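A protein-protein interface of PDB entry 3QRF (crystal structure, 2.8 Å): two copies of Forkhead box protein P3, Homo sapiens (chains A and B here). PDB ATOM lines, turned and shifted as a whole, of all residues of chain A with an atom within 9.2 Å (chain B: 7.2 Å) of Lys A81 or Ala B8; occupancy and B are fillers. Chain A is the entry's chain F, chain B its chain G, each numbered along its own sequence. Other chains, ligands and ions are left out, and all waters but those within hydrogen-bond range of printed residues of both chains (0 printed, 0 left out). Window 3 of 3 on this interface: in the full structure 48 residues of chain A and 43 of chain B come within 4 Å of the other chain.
The side-chain amide nitrogen (ND2) of Asn A53 sits at hydrogen-bond distance from the backbone carbonyl oxygen (O) of Ala A49 (3.1 Å).
A ring nitrogen (NE2) of His A57 sits at hydrogen-bond distance from the side-chain amide oxygen of Asn A53, 2.8 Å away.
NZ of Lys A81 is in hydrogen-bond range of ND1 of His A57, 3.4 Å away.
NH2 of Arg B12 is in salt-bridge range of OE2 of Glu A75, 3.4 Å away.
Of chain B, only Ala B8 comes within 4 Å of Lys A81.
Of chain A, only Asn A53, Phe A60 and Lys A81 come within 4 Å of Ala B8.
No residue of chain A comes within 4 Å of Thr B9.
Of the printed residues of chain A, Tyr B7 touches Ala A49 and Asn A53.
Of the printed residues of chain B, Val A73 touches Arg B12 (3.99 Å).
Of the printed residues of chain B, Phe A60 touches Ala B8.
Printed residues of chain B within 4 Å of Leu A54: Ile B11.
Of the printed residues of chain A, Leu B10 touches Phe A38.
Ala B14 touches none of the printed residues of chain A.
The nearest residue of chain A that does not touch Ala B8 is Phe A78 (4.3 Å).
Printed residues of chain B that touch a printed residue of chain A: Phe B5, Tyr B7, Ala B8, Leu B10, Ile B11, Arg B12 and Phe B32.
Hydrophobic or aromatic side chains of chain B within 4 Å of the printed part of chain A: Tyr B7, Ala B8, Leu B10, Ile B11 and Phe B32.
Printed residues of chain A that touch a printed residue of chain B: Phe A38, Ala A49, Ile A50, Asn A53, Leu A54, Phe A60, Val A73, Glu A75, Phe A78 and Lys A81.
Among the printed residues, Asp or Glu carboxylates within 4 Å of a Lys or Arg side-chain nitrogen of the other chain: Glu A75 with Arg B12 (3.4 Å).
Phe A38 touches Leu B10.
Phe A38 touches Phe B32 (CZ to CE2, 3.6 Å).
CZ of Tyr B7 touches CB of Ala A49, at 3.3 Å.
Phe B32 touches Ile A50.
CB of Tyr B7 touches ND2 of Asn A53 (3.5 Å).
CB of Asn A53 touches CD1 of Ile B11 (3.4 Å).
Phe A60 touches Ala B8 (CZ to O, 3.5 Å).
Val A73 touches Arg B12.
CE2 of Phe A78 touches CD of Arg B12, 3.2 Å away.
Ala B8 touches Lys A81.
No position is printed for both chains.
Of the 15 pairs that touch across the chains among the printed residues, none has its exchanged pair printed and touching as well.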
ATOM      1  N   PHE A  38      -2.396  11.664 -22.700  1.00  0.00           N
ATOM      2  CA  PHE A  38      -2.023  10.388 -22.126  1.00  0.00           C
ATOM      3  C   PHE A  38      -3.236   9.918 -21.378  1.00  0.00           C
ATOM      4  O   PHE A  38      -3.719   8.822 -21.601  1.00  0.00           O
ATOM      5  CB  PHE A  38      -0.869  10.514 -21.134  1.00  0.00           C
ATOM      6  CG  PHE A  38      -0.610   9.248 -20.342  1.00  0.00           C
ATOM      7  CD1 PHE A  38       0.218   8.257 -20.838  1.00  0.00           C
ATOM      8  CD2 PHE A  38      -1.249   9.030 -19.118  1.00  0.00           C
ATOM      9  CE1 PHE A  38       0.403   7.069 -20.135  1.00  0.00           C
ATOM     10  CE2 PHE A  38      -1.071   7.837 -18.401  1.00  0.00           C
ATOM     11  CZ  PHE A  38      -0.247   6.859 -18.912  1.00  0.00           C
ATOM     12  N   ALA A  49       1.156  -2.032 -17.422  1.00  0.00           N
ATOM     13  CA  ALA A  49       2.184  -1.183 -18.015  1.00  0.00           C
ATOM     14  C   ALA A  49       3.091  -0.599 -16.945  1.00  0.00           C
ATOM     15  O   ALA A  49       4.303  -0.492 -17.144  1.00  0.00           O
ATOM     16  CB  ALA A  49       1.552  -0.077 -18.792  1.00  0.00           C
ATOM     17  N   ILE A  50       2.509  -0.223 -15.806  1.00  0.00           N
ATOM     18  CA  ILE A  50       3.290   0.348 -14.714  1.00  0.00           C
ATOM     19  C   ILE A  50       4.166  -0.696 -14.049  1.00  0.00           C
ATOM     20  O   ILE A  50       5.351  -0.463 -13.802  1.00  0.00           O
ATOM     21  CB  ILE A  50       2.401   1.003 -13.655  1.00  0.00           C
ATOM     22  CG1 ILE A  50       1.703   2.211 -14.263  1.00  0.00           C
ATOM     23  CG2 ILE A  50       3.238   1.470 -12.487  1.00  0.00           C
ATOM     24  CD1 ILE A  50       0.908   3.017 -13.280  1.00  0.00           C
ATOM     25  N   HIS A  52       5.199  -3.315 -15.350  1.00  0.00           N
ATOM     26  CA  HIS A  52       6.173  -3.636 -16.384  1.00  0.00           C
ATOM     27  C   HIS A  52       7.360  -2.710 -16.390  1.00  0.00           C
ATOM     28  O   HIS A  52       8.506  -3.164 -16.462  1.00  0.00           O
ATOM     29  CB  HIS A  52       5.552  -3.587 -17.766  1.00  0.00           C
ATOM     30  CG  HIS A  52       6.562  -3.726 -18.861  1.00  0.00           C
ATOM     31  ND1 HIS A  52       7.227  -4.906 -19.113  1.00  0.00           N
ATOM     32  CD2 HIS A  52       7.082  -2.814 -19.717  1.00  0.00           C
ATOM     33  CE1 HIS A  52       8.117  -4.717 -20.073  1.00  0.00           C
ATOM     34  NE2 HIS A  52       8.049  -3.455 -20.457  1.00  0.00           N
ATOM     35  N   ASN A  53       7.069  -1.412 -16.327  1.00  0.00           N
ATOM     36  CA  ASN A  53       8.089  -0.380 -16.351  1.00  0.00           C
ATOM     37  C   ASN A  53       8.926  -0.314 -15.096  1.00  0.00           C
ATOM     38  O   ASN A  53      10.113  -0.006 -15.163  1.00  0.00           O
ATOM     39  CB  ASN A  53       7.434   0.963 -16.571  1.00  0.00           C
ATOM     40  CG  ASN A  53       7.466   1.395 -18.011  1.00  0.00           C
ATOM     41  OD1 ASN A  53       8.381   2.090 -18.429  1.00  0.00           O
ATOM     42  ND2 ASN A  53       6.468   0.981 -18.783  1.00  0.00           N
ATOM     43  N   LEU A  54       8.315  -0.603 -13.950  1.00  0.00           N
ATOM     44  CA  LEU A  54       9.035  -0.533 -12.683  1.00  0.00           C
ATOM     45  C   LEU A  54      10.229  -1.442 -12.603  1.00  0.00           C
ATOM     46  O   LEU A  54      11.294  -1.030 -12.150  1.00  0.00           O
ATOM     47  CB  LEU A  54       8.106  -0.810 -11.508  1.00  0.00           C
ATOM     48  CG  LEU A  54       7.315   0.434 -11.107  1.00  0.00           C
ATOM     49  CD1 LEU A  54       6.304   0.049 -10.066  1.00  0.00           C
ATOM     50  CD2 LEU A  54       8.241   1.516 -10.576  1.00  0.00           C
ATOM     51  N   LEU A  56      11.351  -3.431 -15.377  1.00  0.00           N
ATOM     52  CA  LEU A  56      12.055  -3.382 -16.645  1.00  0.00           C
ATOM     53  C   LEU A  56      13.147  -2.357 -16.645  1.00  0.00           C
ATOM     54  O   LEU A  56      14.257  -2.654 -17.051  1.00  0.00           O
ATOM     55  CB  LEU A  56      11.093  -3.102 -17.794  1.00  0.00           C
ATOM     56  CG  LEU A  56      11.551  -3.314 -19.252  1.00  0.00           C
ATOM     57  CD1 LEU A  56      12.164  -2.029 -19.795  1.00  0.00           C
ATOM     58  CD2 LEU A  56      12.523  -4.498 -19.334  1.00  0.00           C
ATOM     59  N   HIS A  57      12.851  -1.157 -16.161  1.00  0.00           N
ATOM     60  CA  HIS A  57      13.843  -0.083 -16.153  1.00  0.00           C
ATOM     61  C   HIS A  57      14.724  -0.066 -14.930  1.00  0.00           C
ATOM     62  O   HIS A  57      14.235  -0.219 -13.824  1.00  0.00           O
ATOM     63  CB  HIS A  57      13.141   1.263 -16.320  1.00  0.00           C
ATOM     64  CG  HIS A  57      12.431   1.390 -17.628  1.00  0.00           C
ATOM     65  ND1 HIS A  57      13.100   1.378 -18.830  1.00  0.00           N
ATOM     66  CD2 HIS A  57      11.111   1.431 -17.931  1.00  0.00           C
ATOM     67  CE1 HIS A  57      12.221   1.404 -19.818  1.00  0.00           C
ATOM     68  NE2 HIS A  57      11.008   1.434 -19.299  1.00  0.00           N
ATOM     69  N   LYS A  58      16.024   0.122 -15.133  1.00  0.00           N
ATOM     70  CA  LYS A  58      16.980   0.149 -14.023  1.00  0.00           C
ATOM     71  C   LYS A  58      16.890   1.431 -13.222  1.00  0.00           C
ATOM     72  O   LYS A  58      17.665   1.626 -12.295  1.00  0.00           O
ATOM     73  CB  LYS A  58      18.436   0.011 -14.511  1.00  0.00           C
ATOM     74  CG  LYS A  58      18.809  -1.282 -15.265  1.00  0.00           C
ATOM     75  CD  LYS A  58      20.315  -1.306 -15.635  1.00  0.00           C
ATOM     76  CE  LYS A  58      20.667  -2.429 -16.636  1.00  0.00           C
ATOM     77  NZ  LYS A  58      20.174  -2.155 -18.033  1.00  0.00           N
ATOM     78  N   CYS A  59      15.964   2.315 -13.557  1.00  0.00           N
ATOM     79  CA  CYS A  59      15.893   3.555 -12.806  1.00  0.00           C
ATOM     80  C   CYS A  59      14.896   3.491 -11.670  1.00  0.00           C
ATOM     81  O   CYS A  59      14.803   4.426 -10.879  1.00  0.00           O
ATOM     82  CB  CYS A  59      15.554   4.736 -13.725  1.00  0.00           C
ATOM     83  SG  CYS A  59      13.861   4.809 -14.324  1.00  0.00           S
ATOM     84  N   PHE A  60      14.154   2.388 -11.581  1.00  0.00           N
ATOM     85  CA  PHE A  60      13.166   2.227 -10.522  1.00  0.00           C
ATOM     86  C   PHE A  60      13.589   1.068  -9.651  1.00  0.00           C
ATOM     87  O   PHE A  60      13.420  -0.089 -10.024  1.00  0.00           O
ATOM     88  CB  PHE A  60      11.779   1.948 -11.117  1.00  0.00           C
ATOM     89  CG  PHE A  60      11.296   3.017 -12.045  1.00  0.00           C
ATOM     90  CD1 PHE A  60      10.913   2.707 -13.348  1.00  0.00           C
ATOM     91  CD2 PHE A  60      11.293   4.351 -11.648  1.00  0.00           C
ATOM     92  CE1 PHE A  60      10.544   3.713 -14.244  1.00  0.00           C
ATOM     93  CE2 PHE A  60      10.929   5.350 -12.531  1.00  0.00           C
ATOM     94  CZ  PHE A  60      10.555   5.037 -13.833  1.00  0.00           C
ATOM     95  N   VAL A  73      13.267   6.163  -7.144  1.00  0.00           N
ATOM     96  CA  VAL A  73      13.993   6.476  -8.353  1.00  0.00           C
ATOM     97  C   VAL A  73      15.466   6.715  -8.114  1.00  0.00           C
ATOM     98  O   VAL A  73      15.867   7.504  -7.256  1.00  0.00           O
ATOM     99  CB  VAL A  73      13.411   7.715  -9.081  1.00  0.00           C
ATOM    100  CG1 VAL A  73      11.977   7.466  -9.469  1.00  0.00           C
ATOM    101  CG2 VAL A  73      13.504   8.933  -8.190  1.00  0.00           C
ATOM    102  N   ASP A  74      16.264   6.000  -8.890  1.00  0.00           N
ATOM    103  CA  ASP A  74      17.707   6.121  -8.868  1.00  0.00           C
ATOM    104  C   ASP A  74      17.931   7.283  -9.824  1.00  0.00           C
ATOM    105  O   ASP A  74      18.165   7.092 -11.017  1.00  0.00           O
ATOM    106  CB  ASP A  74      18.325   4.850  -9.432  1.00  0.00           C
ATOM    107  CG  ASP A  74      19.815   4.897  -9.456  1.00  0.00           C
ATOM    108  OD1 ASP A  74      20.379   5.863 -10.015  1.00  0.00           O
ATOM    109  OD2 ASP A  74      20.421   3.957  -8.919  1.00  0.00           O
ATOM    110  N   GLU A  75      17.829   8.492  -9.293  1.00  0.00           N
ATOM    111  CA  GLU A  75      17.965   9.697 -10.101  1.00  0.00           C
ATOM    112  C   GLU A  75      18.982   9.661 -11.232  1.00  0.00           C
ATOM    113  O   GLU A  75      18.613   9.763 -12.398  1.00  0.00           O
ATOM    114  CB  GLU A  75      18.262  10.896  -9.211  1.00  0.00           C
ATOM    115  CG  GLU A  75      17.924  12.207  -9.874  1.00  0.00           C
ATOM    116  CD  GLU A  75      16.507  12.211 -10.418  1.00  0.00           C
ATOM    117  OE1 GLU A  75      15.605  11.668  -9.732  1.00  0.00           O
ATOM    118  OE2 GLU A  75      16.297  12.765 -11.522  1.00  0.00           O
ATOM    119  N   LEU A  76      20.259   9.515 -10.891  1.00  0.00           N
ATOM    120  CA  LEU A  76      21.317   9.513 -11.896  1.00  0.00           C
ATOM    121  C   LEU A  76      21.157   8.478 -12.994  1.00  0.00           C
ATOM    122  O   LEU A  76      21.524   8.739 -14.141  1.00  0.00           O
ATOM    123  CB  LEU A  76      22.695   9.379 -11.225  1.00  0.00           C
ATOM    124  CG  LEU A  76      23.268  10.653 -10.560  1.00  0.00           C
ATOM    125  CD1 LEU A  76      22.356  11.140  -9.423  1.00  0.00           C
ATOM    126  CD2 LEU A  76      24.661  10.353 -10.026  1.00  0.00           C
ATOM    127  N   GLU A  77      20.602   7.316 -12.652  1.00  0.00           N
ATOM    128  CA  GLU A  77      20.380   6.250 -13.635  1.00  0.00           C
ATOM    129  C   GLU A  77      19.240   6.644 -14.566  1.00  0.00           C
ATOM    130  O   GLU A  77      19.214   6.266 -15.740  1.00  0.00           O
ATOM    131  CB  GLU A  77      20.036   4.922 -12.937  1.00  0.00           C
ATOM    132  CG  GLU A  77      21.101   3.828 -13.080  1.00  0.00           C
ATOM    133  CD  GLU A  77      21.294   3.356 -14.524  1.00  0.00           C
ATOM    134  OE1 GLU A  77      22.210   2.534 -14.766  1.00  0.00           O
ATOM    135  OE2 GLU A  77      20.533   3.799 -15.417  1.00  0.00           O
ATOM    136  N   PHE A  78      18.300   7.410 -14.029  1.00  0.00           N
ATOM    137  CA  PHE A  78      17.154   7.878 -14.794  1.00  0.00           C
ATOM    138  C   PHE A  78      17.628   8.954 -15.760  1.00  0.00           C
ATOM    139  O   PHE A  78      17.267   8.972 -16.935  1.00  0.00           O
ATOM    140  CB  PHE A  78      16.113   8.465 -13.844  1.00  0.00           C
ATOM    141  CG  PHE A  78      14.960   9.120 -14.536  1.00  0.00           C
ATOM    142  CD1 PHE A  78      13.993   8.356 -15.179  1.00  0.00           C
ATOM    143  CD2 PHE A  78      14.833  10.501 -14.534  1.00  0.00           C
ATOM    144  CE1 PHE A  78      12.909   8.963 -15.809  1.00  0.00           C
ATOM    145  CE2 PHE A  78      13.756  11.117 -15.162  1.00  0.00           C
ATOM    146  CZ  PHE A  78      12.789  10.347 -15.801  1.00  0.00           C
ATOM    147  N   ARG A  79      18.452   9.848 -15.228  1.00  0.00           N
ATOM    148  CA  ARG A  79      19.024  10.959 -15.974  1.00  0.00           C
ATOM    149  C   ARG A  79      19.821  10.438 -17.168  1.00  0.00           C
ATOM    150  O   ARG A  79      19.867  11.073 -18.219  1.00  0.00           O
ATOM    151  CB  ARG A  79      19.930  11.757 -15.044  1.00  0.00           C
ATOM    152  CG  ARG A  79      20.314  13.136 -15.528  1.00  0.00           C
ATOM    153  CD  ARG A  79      21.439  13.673 -14.646  1.00  0.00           C
ATOM    154  NE  ARG A  79      21.236  13.312 -13.241  1.00  0.00           N
ATOM    155  CZ  ARG A  79      22.020  13.705 -12.240  1.00  0.00           C
ATOM    156  NH1 ARG A  79      23.072  14.479 -12.487  1.00  0.00           N
ATOM    157  NH2 ARG A  79      21.747  13.333 -10.991  1.00  0.00           N
ATOM    158  N   LYS A  80      20.453   9.281 -17.000  1.00  0.00           N
ATOM    159  CA  LYS A  80      21.234   8.681 -18.079  1.00  0.00           C
ATOM    160  C   LYS A  80      20.318   8.376 -19.260  1.00  0.00           C
ATOM    161  O   LYS A  80      20.530   8.881 -20.362  1.00  0.00           O
ATOM    162  CB  LYS A  80      21.907   7.391 -17.589  1.00  0.00           C
ATOM    163  CG  LYS A  80      22.952   7.623 -16.502  1.00  0.00           C
ATOM    164  CD  LYS A  80      23.472   6.328 -15.899  1.00  0.00           C
ATOM    165  CE  LYS A  80      24.494   6.626 -14.806  1.00  0.00           C
ATOM    166  NZ  LYS A  80      24.873   5.415 -14.023  1.00  0.00           N
ATOM    167  N   LYS A  81      19.299   7.556 -19.006  1.00  0.00           N
ATOM    168  CA  LYS A  81      18.305   7.145 -20.004  1.00  0.00           C
ATOM    169  C   LYS A  81      18.063   8.189 -21.098  1.00  0.00           C
ATOM    170  O   LYS A  81      18.233   7.898 -22.283  1.00  0.00           O
ATOM    171  CB  LYS A  81      16.975   6.828 -19.305  1.00  0.00           C
ATOM    172  CG  LYS A  81      15.833   6.407 -20.236  1.00  0.00           C
ATOM    173  CD  LYS A  81      14.472   6.853 -19.691  1.00  0.00           C
ATOM    174  CE  LYS A  81      14.071   6.136 -18.411  1.00  0.00           C
ATOM    175  NZ  LYS A  81      13.531   4.776 -18.679  1.00  0.00           N
ATOM    176  N   ARG A  82      17.665   9.396 -20.689  1.00  0.00           N
ATOM    177  CA  ARG A  82      17.379  10.500 -21.611  1.00  0.00           C
ATOM    178  C   ARG A  82      18.302  10.568 -22.829  1.00  0.00           C
ATOM    179  O   ARG A  82      17.779  10.496 -23.964  1.00  0.00           O
ATOM    180  CB  ARG A  82      17.442  11.841 -20.875  1.00  0.00           C
ATOM    181  CG  ARG A  82      16.391  12.042 -19.801  1.00  0.00           C
ATOM    182  CD  ARG A  82      16.352  13.508 -19.401  1.00  0.00           C
ATOM    183  NE  ARG A  82      15.302  13.818 -18.433  1.00  0.00           N
ATOM    184  CZ  ARG A  82      14.935  15.057 -18.108  1.00  0.00           C
ATOM    185  NH1 ARG A  82      15.534  16.098 -18.676  1.00  0.00           N
ATOM    186  NH2 ARG A  82      13.970  15.258 -17.219  1.00  0.00           N
ATOM    187  OXT ARG A  82      19.533  10.705 -22.642  1.00  0.00           O
ATOM    188  N   PHE B   5       3.928  11.967 -22.245  1.00  0.00           N
ATOM    189  CA  PHE B   5       5.026  11.625 -21.390  1.00  0.00           C
ATOM    190  C   PHE B   5       4.953  10.091 -21.285  1.00  0.00           C
ATOM    191  O   PHE B   5       3.878   9.510 -21.062  1.00  0.00           O
ATOM    192  CB  PHE B   5       4.801  12.224 -20.014  1.00  0.00           C
ATOM    193  CG  PHE B   5       4.560  13.690 -20.026  1.00  0.00           C
ATOM    194  CD1 PHE B   5       3.425  14.219 -19.422  1.00  0.00           C
ATOM    195  CD2 PHE B   5       5.493  14.553 -20.580  1.00  0.00           C
ATOM    196  CE1 PHE B   5       3.225  15.586 -19.363  1.00  0.00           C
ATOM    197  CE2 PHE B   5       5.307  15.922 -20.530  1.00  0.00           C
ATOM    198  CZ  PHE B   5       4.170  16.441 -19.918  1.00  0.00           C
ATOM    199  N   THR B   6       6.088   9.437 -21.453  1.00  0.00           N
ATOM    200  CA  THR B   6       6.138   7.997 -21.366  1.00  0.00           C
ATOM    201  C   THR B   6       5.849   7.567 -19.935  1.00  0.00           C
ATOM    202  O   THR B   6       5.797   8.394 -19.030  1.00  0.00           O
ATOM    203  CB  THR B   6       7.501   7.526 -21.728  1.00  0.00           C
ATOM    204  OG1 THR B   6       8.444   8.127 -20.830  1.00  0.00           O
ATOM    205  CG2 THR B   6       7.822   7.938 -23.152  1.00  0.00           C
ATOM    206  N   TYR B   7       5.665   6.268 -19.732  1.00  0.00           N
ATOM    207  CA  TYR B   7       5.389   5.742 -18.414  1.00  0.00           C
ATOM    208  C   TYR B   7       6.462   6.122 -17.403  1.00  0.00           C
ATOM    209  O   TYR B   7       6.152   6.646 -16.339  1.00  0.00           O
ATOM    210  CB  TYR B   7       5.256   4.218 -18.464  1.00  0.00           C
ATOM    211  CG  TYR B   7       3.900   3.749 -18.923  1.00  0.00           C
ATOM    212  CD1 TYR B   7       3.604   3.587 -20.283  1.00  0.00           C
ATOM    213  CD2 TYR B   7       2.881   3.544 -17.995  1.00  0.00           C
ATOM    214  CE1 TYR B   7       2.324   3.238 -20.699  1.00  0.00           C
ATOM    215  CE2 TYR B   7       1.602   3.199 -18.392  1.00  0.00           C
ATOM    216  CZ  TYR B   7       1.320   3.048 -19.742  1.00  0.00           C
ATOM    217  OH  TYR B   7       0.029   2.713 -20.102  1.00  0.00           O
ATOM    218  N   ALA B   8       7.722   5.871 -17.726  1.00  0.00           N
ATOM    219  CA  ALA B   8       8.799   6.179 -16.803  1.00  0.00           C
ATOM    220  C   ALA B   8       8.694   7.609 -16.284  1.00  0.00           C
ATOM    221  O   ALA B   8       8.853   7.873 -15.081  1.00  0.00           O
ATOM    222  CB  ALA B   8      10.135   5.966 -17.481  1.00  0.00           C
ATOM    223  N   THR B   9       8.431   8.538 -17.190  1.00  0.00           N
ATOM    224  CA  THR B   9       8.312   9.922 -16.791  1.00  0.00           C
ATOM    225  C   THR B   9       7.189  10.023 -15.778  1.00  0.00           C
ATOM    226  O   THR B   9       7.361  10.574 -14.682  1.00  0.00           O
ATOM    227  CB  THR B   9       7.967  10.830 -17.974  1.00  0.00           C
ATOM    228  OG1 THR B   9       9.059  10.878 -18.887  1.00  0.00           O
ATOM    229  CG2 THR B   9       7.663  12.220 -17.487  1.00  0.00           C
ATOM    230  N   LEU B  10       6.028   9.483 -16.130  1.00  0.00           N
ATOM    231  CA  LEU B  10       4.901   9.566 -15.226  1.00  0.00           C
ATOM    232  C   LEU B  10       5.173   8.814 -13.919  1.00  0.00           C
ATOM    233  O   LEU B  10       5.007   9.368 -12.830  1.00  0.00           O
ATOM    234  CB  LEU B  10       3.653   9.041 -15.925  1.00  0.00           C
ATOM    235  CG  LEU B  10       3.271   9.867 -17.156  1.00  0.00           C
ATOM    236  CD1 LEU B  10       2.339   9.102 -18.089  1.00  0.00           C
ATOM    237  CD2 LEU B  10       2.610  11.118 -16.699  1.00  0.00           C
ATOM    238  N   ILE B  11       5.616   7.563 -14.027  1.00  0.00           N
ATOM    239  CA  ILE B  11       5.898   6.751 -12.847  1.00  0.00           C
ATOM    240  C   ILE B  11       6.877   7.466 -11.916  1.00  0.00           C
ATOM    241  O   ILE B  11       6.718   7.422 -10.685  1.00  0.00           O
ATOM    242  CB  ILE B  11       6.465   5.377 -13.239  1.00  0.00           C
ATOM    243  CG1 ILE B  11       5.436   4.617 -14.067  1.00  0.00           C
ATOM    244  CG2 ILE B  11       6.776   4.576 -12.009  1.00  0.00           C
ATOM    245  CD1 ILE B  11       5.940   3.306 -14.629  1.00  0.00           C
ATOM    246  N   ARG B  12       7.887   8.119 -12.492  1.00  0.00           N
ATOM    247  CA  ARG B  12       8.843   8.859 -11.676  1.00  0.00           C
ATOM    248  C   ARG B  12       8.137   9.989 -10.929  1.00  0.00           C
ATOM    249  O   ARG B  12       8.296  10.134  -9.708  1.00  0.00           O
ATOM    250  CB  ARG B  12       9.953   9.467 -12.527  1.00  0.00           C
ATOM    251  CG  ARG B  12      10.783  10.502 -11.771  1.00  0.00           C
ATOM    252  CD  ARG B  12      12.116  10.744 -12.470  1.00  0.00           C
ATOM    253  NE  ARG B  12      12.853  11.877 -11.910  1.00  0.00           N
ATOM    254  CZ  ARG B  12      12.452  13.143 -11.992  1.00  0.00           C
ATOM    255  NH1 ARG B  12      11.318  13.444 -12.620  1.00  0.00           N
ATOM    256  NH2 ARG B  12      13.169  14.103 -11.425  1.00  0.00           N
ATOM    257  N   TRP B  13       7.359  10.793 -11.655  1.00  0.00           N
ATOM    258  CA  TRP B  13       6.665  11.875 -10.992  1.00  0.00           C
ATOM    259  C   TRP B  13       5.832  11.345  -9.837  1.00  0.00           C
ATOM    260  O   TRP B  13       5.808  11.935  -8.764  1.00  0.00           O
ATOM    261  CB  TRP B  13       5.753  12.637 -11.948  1.00  0.00           C
ATOM    262  CG  TRP B  13       6.447  13.552 -12.872  1.00  0.00           C
ATOM    263  CD1 TRP B  13       7.666  14.114 -12.698  1.00  0.00           C
ATOM    264  CD2 TRP B  13       5.980  13.988 -14.154  1.00  0.00           C
ATOM    265  NE1 TRP B  13       8.010  14.871 -13.802  1.00  0.00           N
ATOM    266  CE2 TRP B  13       6.990  14.812 -14.709  1.00  0.00           C
ATOM    267  CE3 TRP B  13       4.807  13.762 -14.887  1.00  0.00           C
ATOM    268  CZ2 TRP B  13       6.869  15.409 -15.965  1.00  0.00           C
ATOM    269  CZ3 TRP B  13       4.684  14.357 -16.140  1.00  0.00           C
ATOM    270  CH2 TRP B  13       5.714  15.173 -16.667  1.00  0.00           C
ATOM    271  N   ALA B  14       5.152  10.229 -10.049  1.00  0.00           N
ATOM    272  CA  ALA B  14       4.308   9.675  -9.002  1.00  0.00           C
ATOM    273  C   ALA B  14       5.117   9.299  -7.775  1.00  0.00           C
ATOM    274  O   ALA B  14       4.616   9.323  -6.652  1.00  0.00           O
ATOM    275  CB  ALA B  14       3.547   8.475  -9.527  1.00  0.00           C
ATOM    276  N   PHE B  32      -1.815   7.797 -10.452  1.00  0.00           N
ATOM    277  CA  PHE B  32      -2.345   7.751 -11.810  1.00  0.00           C
ATOM    278  C   PHE B  32      -3.865   7.956 -11.835  1.00  0.00           C
ATOM    279  O   PHE B  32      -4.397   8.664 -12.695  1.00  0.00           O
ATOM    280  CB  PHE B  32      -2.042   6.410 -12.469  1.00  0.00           C
ATOM    281  CG  PHE B  32      -0.773   6.395 -13.249  1.00  0.00           C
ATOM    282  CD1 PHE B  32       0.461   6.421 -12.602  1.00  0.00           C
ATOM    283  CD2 PHE B  32      -0.805   6.382 -14.644  1.00  0.00           C
ATOM    284  CE1 PHE B  32       1.637   6.438 -13.332  1.00  0.00           C
ATOM    285  CE2 PHE B  32       0.367   6.400 -15.372  1.00  0.00           C
ATOM    286  CZ  PHE B  32       1.595   6.430 -14.711  1.00  0.00           C
